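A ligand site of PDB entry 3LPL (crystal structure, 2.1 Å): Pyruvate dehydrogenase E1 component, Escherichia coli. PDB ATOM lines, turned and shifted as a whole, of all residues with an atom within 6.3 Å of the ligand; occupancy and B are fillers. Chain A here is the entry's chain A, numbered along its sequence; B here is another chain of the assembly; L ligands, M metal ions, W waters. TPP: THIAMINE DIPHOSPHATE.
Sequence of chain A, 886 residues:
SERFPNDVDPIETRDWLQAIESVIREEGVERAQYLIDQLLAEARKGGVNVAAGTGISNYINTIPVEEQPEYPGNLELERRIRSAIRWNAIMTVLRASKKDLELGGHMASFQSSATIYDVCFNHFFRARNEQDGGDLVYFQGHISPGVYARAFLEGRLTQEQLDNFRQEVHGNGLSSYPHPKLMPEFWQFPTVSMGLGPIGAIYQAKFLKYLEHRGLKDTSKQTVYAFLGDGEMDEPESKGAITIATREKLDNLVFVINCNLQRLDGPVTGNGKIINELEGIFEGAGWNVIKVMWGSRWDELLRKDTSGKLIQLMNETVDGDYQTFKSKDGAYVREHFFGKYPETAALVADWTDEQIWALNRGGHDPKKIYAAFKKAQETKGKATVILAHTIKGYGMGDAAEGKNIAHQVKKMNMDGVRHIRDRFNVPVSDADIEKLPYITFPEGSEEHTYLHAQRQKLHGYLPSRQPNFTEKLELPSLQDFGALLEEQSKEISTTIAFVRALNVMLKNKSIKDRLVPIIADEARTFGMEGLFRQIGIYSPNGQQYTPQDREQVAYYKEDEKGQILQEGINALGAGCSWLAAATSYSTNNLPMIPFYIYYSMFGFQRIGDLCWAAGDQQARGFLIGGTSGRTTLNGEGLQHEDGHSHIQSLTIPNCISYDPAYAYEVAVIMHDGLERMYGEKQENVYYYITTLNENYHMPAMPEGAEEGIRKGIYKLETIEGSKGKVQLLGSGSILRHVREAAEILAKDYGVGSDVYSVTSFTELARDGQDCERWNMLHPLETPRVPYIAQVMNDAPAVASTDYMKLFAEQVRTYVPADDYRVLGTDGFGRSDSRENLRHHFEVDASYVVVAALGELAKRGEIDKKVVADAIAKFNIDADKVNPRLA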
ATOM      1  N   ALA A 108      -5.143  -1.045 -32.741  1.00  0.00           N
ATOM      2  CA  ALA A 108      -6.161  -1.078 -33.794  1.00  0.00           C
ATOM      3  C   ALA A 108      -7.194   0.058 -33.726  1.00  0.00           C
ATOM      4  O   ALA A 108      -7.497   0.722 -34.728  1.00  0.00           O
ATOM      5  CB  ALA A 108      -6.878  -2.433 -33.785  1.00  0.00           C
ATOM      6  N   SER A 109      -7.743   0.264 -32.533  1.00  0.00           N
ATOM      7  CA  SER A 109      -8.751   1.282 -32.357  1.00  0.00           C
ATOM      8  C   SER A 109      -8.305   2.702 -32.751  1.00  0.00           C
ATOM      9  O   SER A 109      -8.947   3.345 -33.576  1.00  0.00           O
ATOM     10  CB  SER A 109      -9.231   1.285 -30.923  1.00  0.00           C
ATOM     11  OG  SER A 109     -10.356   2.115 -30.822  1.00  0.00           O
ATOM     12  N   SER A 112      -8.058   3.419 -36.420  1.00  0.00           N
ATOM     13  CA  SER A 112      -9.256   3.628 -37.198  1.00  0.00           C
ATOM     14  C   SER A 112      -9.867   5.010 -36.953  1.00  0.00           C
ATOM     15  O   SER A 112     -10.643   5.486 -37.752  1.00  0.00           O
ATOM     16  CB  SER A 112     -10.307   2.523 -36.945  1.00  0.00           C
ATOM     17  OG  SER A 112     -10.784   2.496 -35.619  1.00  0.00           O
ATOM     18  N   GLN A 140     -12.206   8.433 -26.129  1.00  0.00           N
ATOM     19  CA  GLN A 140     -12.466   7.010 -26.013  1.00  0.00           C
ATOM     20  C   GLN A 140     -11.224   6.446 -25.326  1.00  0.00           C
ATOM     21  O   GLN A 140     -10.102   6.597 -25.816  1.00  0.00           O
ATOM     22  CB  GLN A 140     -12.660   6.426 -27.411  1.00  0.00           C
ATOM     23  CG  GLN A 140     -12.893   4.936 -27.464  1.00  0.00           C
ATOM     24  CD  GLN A 140     -13.232   4.468 -28.865  1.00  0.00           C
ATOM     25  OE1 GLN A 140     -12.746   5.053 -29.844  1.00  0.00           O
ATOM     26  NE2 GLN A 140     -14.057   3.424 -28.984  1.00  0.00           N
ATOM     27  N   HIS A 142      -9.642   3.522 -24.908  1.00  0.00           N
ATOM     28  CA  HIS A 142      -8.709   2.641 -25.584  1.00  0.00           C
ATOM     29  C   HIS A 142      -7.760   3.332 -26.570  1.00  0.00           C
ATOM     30  O   HIS A 142      -6.791   2.717 -27.015  1.00  0.00           O
ATOM     31  CB  HIS A 142      -9.456   1.520 -26.317  1.00  0.00           C
ATOM     32  CG  HIS A 142     -10.098   0.522 -25.407  1.00  0.00           C
ATOM     33  ND1 HIS A 142      -9.743   0.380 -24.081  1.00  0.00           N
ATOM     34  CD2 HIS A 142     -11.050  -0.419 -25.637  1.00  0.00           C
ATOM     35  CE1 HIS A 142     -10.440  -0.595 -23.533  1.00  0.00           C
ATOM     36  NE2 HIS A 142     -11.237  -1.106 -24.456  1.00  0.00           N
ATOM     37  N   MET A 194     -17.147   1.473 -20.338  1.00  0.00           N
ATOM     38  CA  MET A 194     -18.102   1.746 -21.420  1.00  0.00           C
ATOM     39  C   MET A 194     -19.496   2.165 -20.959  1.00  0.00           C
ATOM     40  O   MET A 194     -20.030   1.625 -19.989  1.00  0.00           O
ATOM     41  CB  MET A 194     -18.235   0.520 -22.322  1.00  0.00           C
ATOM     42  CG  MET A 194     -16.951  -0.237 -22.576  1.00  0.00           C
ATOM     43  SD  MET A 194     -16.207   0.096 -24.194  1.00  0.00           S
ATOM     44  CE  MET A 194     -15.565   1.716 -23.772  1.00  0.00           C
ATOM     45  N   LEU A 228     -17.334   7.822 -28.779  1.00  0.00           N
ATOM     46  CA  LEU A 228     -17.810   6.470 -28.468  1.00  0.00           C
ATOM     47  C   LEU A 228     -17.484   5.447 -29.532  1.00  0.00           C
ATOM     48  O   LEU A 228     -17.116   5.801 -30.664  1.00  0.00           O
ATOM     49  CB  LEU A 228     -19.327   6.517 -28.325  1.00  0.00           C
ATOM     50  CG  LEU A 228     -19.770   7.735 -27.492  1.00  0.00           C
ATOM     51  CD1 LEU A 228     -21.259   7.970 -27.615  1.00  0.00           C
ATOM     52  CD2 LEU A 228     -19.340   7.533 -26.026  1.00  0.00           C
ATOM     53  N   GLY A 229     -17.655   4.179 -29.179  1.00  0.00           N
ATOM     54  CA  GLY A 229     -17.449   3.094 -30.111  1.00  0.00           C
ATOM     55  C   GLY A 229     -18.828   2.565 -30.481  1.00  0.00           C
ATOM     56  O   GLY A 229     -19.772   2.732 -29.699  1.00  0.00           O
ATOM     57  N   ASP A 230     -18.974   1.943 -31.649  1.00  0.00           N
ATOM     58  CA  ASP A 230     -20.297   1.448 -31.994  1.00  0.00           C
ATOM     59  C   ASP A 230     -20.677   0.248 -31.116  1.00  0.00           C
ATOM     60  O   ASP A 230     -21.854   0.070 -30.779  1.00  0.00           O
ATOM     61  CB  ASP A 230     -20.427   1.144 -33.499  1.00  0.00           C
ATOM     62  CG  ASP A 230     -19.294   0.263 -34.036  1.00  0.00           C
ATOM     63  OD1 ASP A 230     -18.236   0.150 -33.412  1.00  0.00           O
ATOM     64  OD2 ASP A 230     -19.463  -0.312 -35.134  1.00  0.00           O
ATOM     65  N   GLY A 231     -19.678  -0.537 -30.709  1.00  0.00           N
ATOM     66  CA  GLY A 231     -19.936  -1.660 -29.816  1.00  0.00           C
ATOM     67  C   GLY A 231     -20.397  -1.146 -28.453  1.00  0.00           C
ATOM     68  O   GLY A 231     -21.280  -1.731 -27.822  1.00  0.00           O
ATOM     69  N   GLU A 232     -19.819  -0.022 -28.023  1.00  0.00           N
ATOM     70  CA  GLU A 232     -20.166   0.574 -26.746  1.00  0.00           C
ATOM     71  C   GLU A 232     -21.632   1.043 -26.675  1.00  0.00           C
ATOM     72  O   GLU A 232     -22.245   1.068 -25.597  1.00  0.00           O
ATOM     73  CB  GLU A 232     -19.199   1.735 -26.457  1.00  0.00           C
ATOM     74  CG  GLU A 232     -19.696   2.757 -25.430  1.00  0.00           C
ATOM     75  CD  GLU A 232     -18.606   3.711 -24.963  1.00  0.00           C
ATOM     76  OE1 GLU A 232     -17.715   4.069 -25.782  1.00  0.00           O
ATOM     77  OE2 GLU A 232     -18.634   4.111 -23.772  1.00  0.00           O
ATOM     78  N   MET A 233     -22.220   1.377 -27.821  1.00  0.00           N
ATOM     79  CA  MET A 233     -23.608   1.820 -27.836  1.00  0.00           C
ATOM     80  C   MET A 233     -24.635   0.785 -27.309  1.00  0.00           C
ATOM     81  O   MET A 233     -25.784   1.137 -26.999  1.00  0.00           O
ATOM     82  CB  MET A 233     -23.982   2.308 -29.229  1.00  0.00           C
ATOM     83  CG  MET A 233     -23.028   3.374 -29.775  1.00  0.00           C
ATOM     84  SD  MET A 233     -22.689   4.763 -28.628  1.00  0.00           S
ATOM     85  CE  MET A 233     -24.389   5.448 -28.436  1.00  0.00           C
ATOM     86  N   ASN A 258     -17.609   6.081 -33.491  1.00  0.00           N
ATOM     87  CA  ASN A 258     -16.711   5.452 -34.438  1.00  0.00           C
ATOM     88  C   ASN A 258     -17.373   4.143 -34.876  1.00  0.00           C
ATOM     89  O   ASN A 258     -17.471   3.184 -34.122  1.00  0.00           O
ATOM     90  CB  ASN A 258     -15.354   5.207 -33.774  1.00  0.00           C
ATOM     91  CG  ASN A 258     -14.363   4.564 -34.716  1.00  0.00           C
ATOM     92  OD1 ASN A 258     -14.641   4.413 -35.896  1.00  0.00           O
ATOM     93  ND2 ASN A 258     -13.185   4.202 -34.192  1.00  0.00           N
ATOM     94  N   ASN A 260     -16.843   1.339 -36.900  1.00  0.00           N
ATOM     95  CA  ASN A 260     -15.968   0.478 -37.674  1.00  0.00           C
ATOM     96  C   ASN A 260     -16.664  -0.863 -37.816  1.00  0.00           C
ATOM     97  O   ASN A 260     -16.062  -1.851 -38.219  1.00  0.00           O
ATOM     98  CB  ASN A 260     -14.585   0.320 -37.017  1.00  0.00           C
ATOM     99  CG  ASN A 260     -14.658   0.215 -35.506  1.00  0.00           C
ATOM    100  OD1 ASN A 260     -15.552  -0.430 -34.968  1.00  0.00           O
ATOM    101  ND2 ASN A 260     -13.706   0.831 -34.827  1.00  0.00           N
ATOM    102  N   GLN A 262     -17.233  -3.025 -36.029  1.00  0.00           N
ATOM    103  CA  GLN A 262     -16.662  -4.041 -35.152  1.00  0.00           C
ATOM    104  C   GLN A 262     -16.655  -3.654 -33.681  1.00  0.00           C
ATOM    105  O   GLN A 262     -16.625  -2.454 -33.303  1.00  0.00           O
ATOM    106  CB  GLN A 262     -15.189  -4.353 -35.514  1.00  0.00           C
ATOM    107  CG  GLN A 262     -14.841  -4.692 -36.978  1.00  0.00           C
ATOM    108  CD  GLN A 262     -13.354  -5.134 -37.160  1.00  0.00           C
ATOM    109  OE1 GLN A 262     -12.717  -4.839 -38.198  1.00  0.00           O
ATOM    110  NE2 GLN A 262     -12.811  -5.846 -36.158  1.00  0.00           N
ATOM    111  N   ARG A 263     -16.681  -4.663 -32.819  1.00  0.00           N
ATOM    112  CA  ARG A 263     -16.490  -4.443 -31.394  1.00  0.00           C
ATOM    113  C   ARG A 263     -15.136  -5.054 -31.070  1.00  0.00           C
ATOM    114  O   ARG A 263     -14.186  -4.908 -31.842  1.00  0.00           O
ATOM    115  CB  ARG A 263     -17.591  -5.138 -30.598  1.00  0.00           C
ATOM    116  CG  ARG A 263     -17.572  -6.650 -30.682  1.00  0.00           C
ATOM    117  CD  ARG A 263     -18.756  -7.270 -29.945  1.00  0.00           C
ATOM    118  NE  ARG A 263     -18.726  -8.728 -29.983  1.00  0.00           N
ATOM    119  CZ  ARG A 263     -19.178  -9.454 -30.998  1.00  0.00           C
ATOM    120  NH1 ARG A 263     -19.703  -8.871 -32.063  1.00  0.00           N
ATOM    121  NH2 ARG A 263     -19.106 -10.779 -30.949  1.00  0.00           N
ATOM    122  N   LEU A 264     -15.053  -5.755 -29.943  1.00  0.00           N
ATOM    123  CA  LEU A 264     -13.862  -6.570 -29.675  1.00  0.00           C
ATOM    124  C   LEU A 264     -13.796  -7.952 -30.334  1.00  0.00           C
ATOM    125  O   LEU A 264     -12.917  -8.188 -31.184  1.00  0.00           O
ATOM    126  CB  LEU A 264     -13.681  -6.723 -28.167  1.00  0.00           C
ATOM    127  CG  LEU A 264     -12.235  -6.809 -27.639  1.00  0.00           C
ATOM    128  CD1 LEU A 264     -11.281  -7.232 -28.771  1.00  0.00           C
ATOM    129  CD2 LEU A 264     -11.820  -5.444 -27.059  1.00  0.00           C
ATOM    130  N   VAL A 268     -20.652  -5.555 -34.413  1.00  0.00           N
ATOM    131  CA  VAL A 268     -21.795  -5.195 -33.559  1.00  0.00           C
ATOM    132  C   VAL A 268     -23.019  -6.051 -33.913  1.00  0.00           C
ATOM    133  O   VAL A 268     -23.547  -6.783 -33.061  1.00  0.00           O
ATOM    134  CB  VAL A 268     -22.175  -3.696 -33.718  1.00  0.00           C
ATOM    135  CG1 VAL A 268     -23.162  -3.302 -32.609  1.00  0.00           C
ATOM    136  CG2 VAL A 268     -20.926  -2.822 -33.673  1.00  0.00           C
ATOM    137  N   LYS A 392     -11.579  -0.741 -38.952  1.00  0.00           N
ATOM    138  CA  LYS A 392     -10.850  -1.143 -37.747  1.00  0.00           C
ATOM    139  C   LYS A 392      -9.515  -1.787 -38.134  1.00  0.00           C
ATOM    140  O   LYS A 392      -9.451  -2.634 -39.014  1.00  0.00           O
ATOM    141  CB  LYS A 392     -11.690  -2.130 -36.915  1.00  0.00           C
ATOM    142  CG  LYS A 392     -11.022  -2.534 -35.597  1.00  0.00           C
ATOM    143  CD  LYS A 392     -11.924  -3.474 -34.771  1.00  0.00           C
ATOM    144  CE  LYS A 392     -11.247  -3.900 -33.474  1.00  0.00           C
ATOM    145  NZ  LYS A 392     -12.133  -4.814 -32.693  1.00  0.00           N
ATOM    146  N   ASP B 521     -19.612  -9.943 -25.108  1.00  0.00           N
ATOM    147  CA  ASP B 521     -18.621  -9.709 -26.155  1.00  0.00           C
ATOM    148  C   ASP B 521     -17.375 -10.543 -25.844  1.00  0.00           C
ATOM    149  O   ASP B 521     -17.190 -11.629 -26.412  1.00  0.00           O
ATOM    150  CB  ASP B 521     -18.244  -8.209 -26.243  1.00  0.00           C
ATOM    151  CG  ASP B 521     -17.195  -7.920 -27.355  1.00  0.00           C
ATOM    152  OD1 ASP B 521     -16.993  -8.793 -28.259  1.00  0.00           O
ATOM    153  OD2 ASP B 521     -16.588  -6.822 -27.327  1.00  0.00           O
ATOM    154  N   GLU B 522     -16.538 -10.015 -24.950  1.00  0.00           N
ATOM    155  CA  GLU B 522     -15.295 -10.630 -24.510  1.00  0.00           C
ATOM    156  C   GLU B 522     -15.305 -12.146 -24.407  1.00  0.00           C
ATOM    157  O   GLU B 522     -15.849 -12.726 -23.444  1.00  0.00           O
ATOM    158  CB  GLU B 522     -14.914 -10.055 -23.152  1.00  0.00           C
ATOM    159  CG  GLU B 522     -14.583  -8.568 -23.206  1.00  0.00           C
ATOM    160  CD  GLU B 522     -13.459  -8.271 -24.158  1.00  0.00           C
ATOM    161  OE1 GLU B 522     -12.500  -9.068 -24.186  1.00  0.00           O
ATOM    162  OE2 GLU B 522     -13.539  -7.244 -24.886  1.00  0.00           O
ATOM    163  N   ILE B 569     -21.214  -5.667 -25.705  1.00  0.00           N
ATOM    164  CA  ILE B 569     -20.703  -4.842 -24.622  1.00  0.00           C
ATOM    165  C   ILE B 569     -21.967  -4.324 -23.911  1.00  0.00           C
ATOM    166  O   ILE B 569     -22.398  -3.194 -24.124  1.00  0.00           O
ATOM    167  CB  ILE B 569     -19.872  -3.687 -25.210  1.00  0.00           C
ATOM    168  CG1 ILE B 569     -18.834  -4.278 -26.190  1.00  0.00           C
ATOM    169  CG2 ILE B 569     -19.208  -2.875 -24.059  1.00  0.00           C
ATOM    170  CD1 ILE B 569     -18.002  -3.245 -26.954  1.00  0.00           C
HETATM  171  C6  TPP L   1     -14.212  -3.057 -27.081  1.00  0.00           C
HETATM  172  C7  TPP L   1     -14.859  -1.757 -27.549  1.00  0.00           C
HETATM  173  O7  TPP L   1     -15.475  -1.896 -28.831  1.00  0.00           O
HETATM  174  PA  TPP L   1     -16.098  -0.595 -29.557  1.00  0.00           P
HETATM  175  O1A TPP L   1     -16.982   0.102 -28.592  1.00  0.00           O
HETATM  176  O2A TPP L   1     -16.674  -1.022 -30.844  1.00  0.00           O
HETATM  177  O3A TPP L   1     -14.778   0.322 -29.763  1.00  0.00           O
HETATM  178  PB  TPP L   1     -13.771   0.162 -31.014  1.00  0.00           P
HETATM  179  O1B TPP L   1     -12.410  -0.485 -30.454  1.00  0.00           O
HETATM  180  O2B TPP L   1     -13.529   1.473 -31.672  1.00  0.00           O
HETATM  181  O3B TPP L   1     -14.426  -0.923 -32.005  1.00  0.00           O
HETATM  182 MG    MG M   1     -16.009   1.079 -32.855  1.00  0.00          MG
HETATM  183  O   HOH W   1     -15.716   2.584 -26.971  1.00  0.00           O
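Water W1 lies within hydrogen-bond range of the side-chain amide nitrogen (NE2) of Gln 140 (2.7 Å), the side-chain carboxylate (OE1) of Glu 232 (2.8 Å), an oxygen (O1A) of the ligand (3.2 Å), the backbone NH (N) of Gly 229 (3.3 Å) and the side-chain sulfur (SD) of Met 194 (3.8 Å).
The side-chain carboxylate (OD1) of Asp 230 sits close to an oxygen (O2A) of the ligand. CA of Gly 229 touches O1A of the ligand, at 3.4 Å. Asn 258 touches the ligand (ND2 to O2B, 3.7 Å). Arg 263 touches the ligand (CA to O2A, 3.5 Å). Leu 264 touches the ligand (CD2 to C6, 3.4 Å). Ile 569 of chain B touches the ligand.
O2A of the ligand lies close to O of Gln 262 (2.8 Å). An oxygen (O1A) of the ligand lies within hydrogen-bond range of the backbone NH of Glu 232 (2.9 Å). The backbone NH (N) of Gly 231 sits at hydrogen-bond distance from an oxygen (O2A) of the ligand (3.0 Å). OD1 of Asn 260 lies close to O3B of the ligand (3.2 Å). The side-chain amide nitrogen (NE2) of Gln 140 is in hydrogen-bond range of an oxygen (O3A) of the ligand. The side-chain hydroxyl (OG) of Ser 109 is in hydrogen-bond range of an oxygen (O1B) of the ligand (3.3 Å).
The backbone NH (N) of Gly 229 lies within hydrogen-bond range of the side-chain carboxylate (OE1) of Glu 232, 3.4 Å away. The side-chain amide oxygen (OD1) of Asn 260 lies close to the side-chain carboxylate (OD1) of Asp 230. ND2 of Asn 260 lies close to ND2 of Asn 258, 3.5 Å away. The side-chain hydroxyl (OG) of Ser 112 lies within hydrogen-bond range of the side-chain amide nitrogen (ND2) of Asn 260. O of Asn 258 is in hydrogen-bond range of N of Asp 230, 3.1 Å away. O of Ser 109 is in hydrogen-bond range of OG of Ser 112. The side-chain amide nitrogen (ND2) of Asn 258 is in hydrogen-bond range of the side-chain hydroxyl (OG) of Ser 112, at 3.3 Å. O of Leu 228 lies within hydrogen-bond range of N of Asn 258 (2.9 Å).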
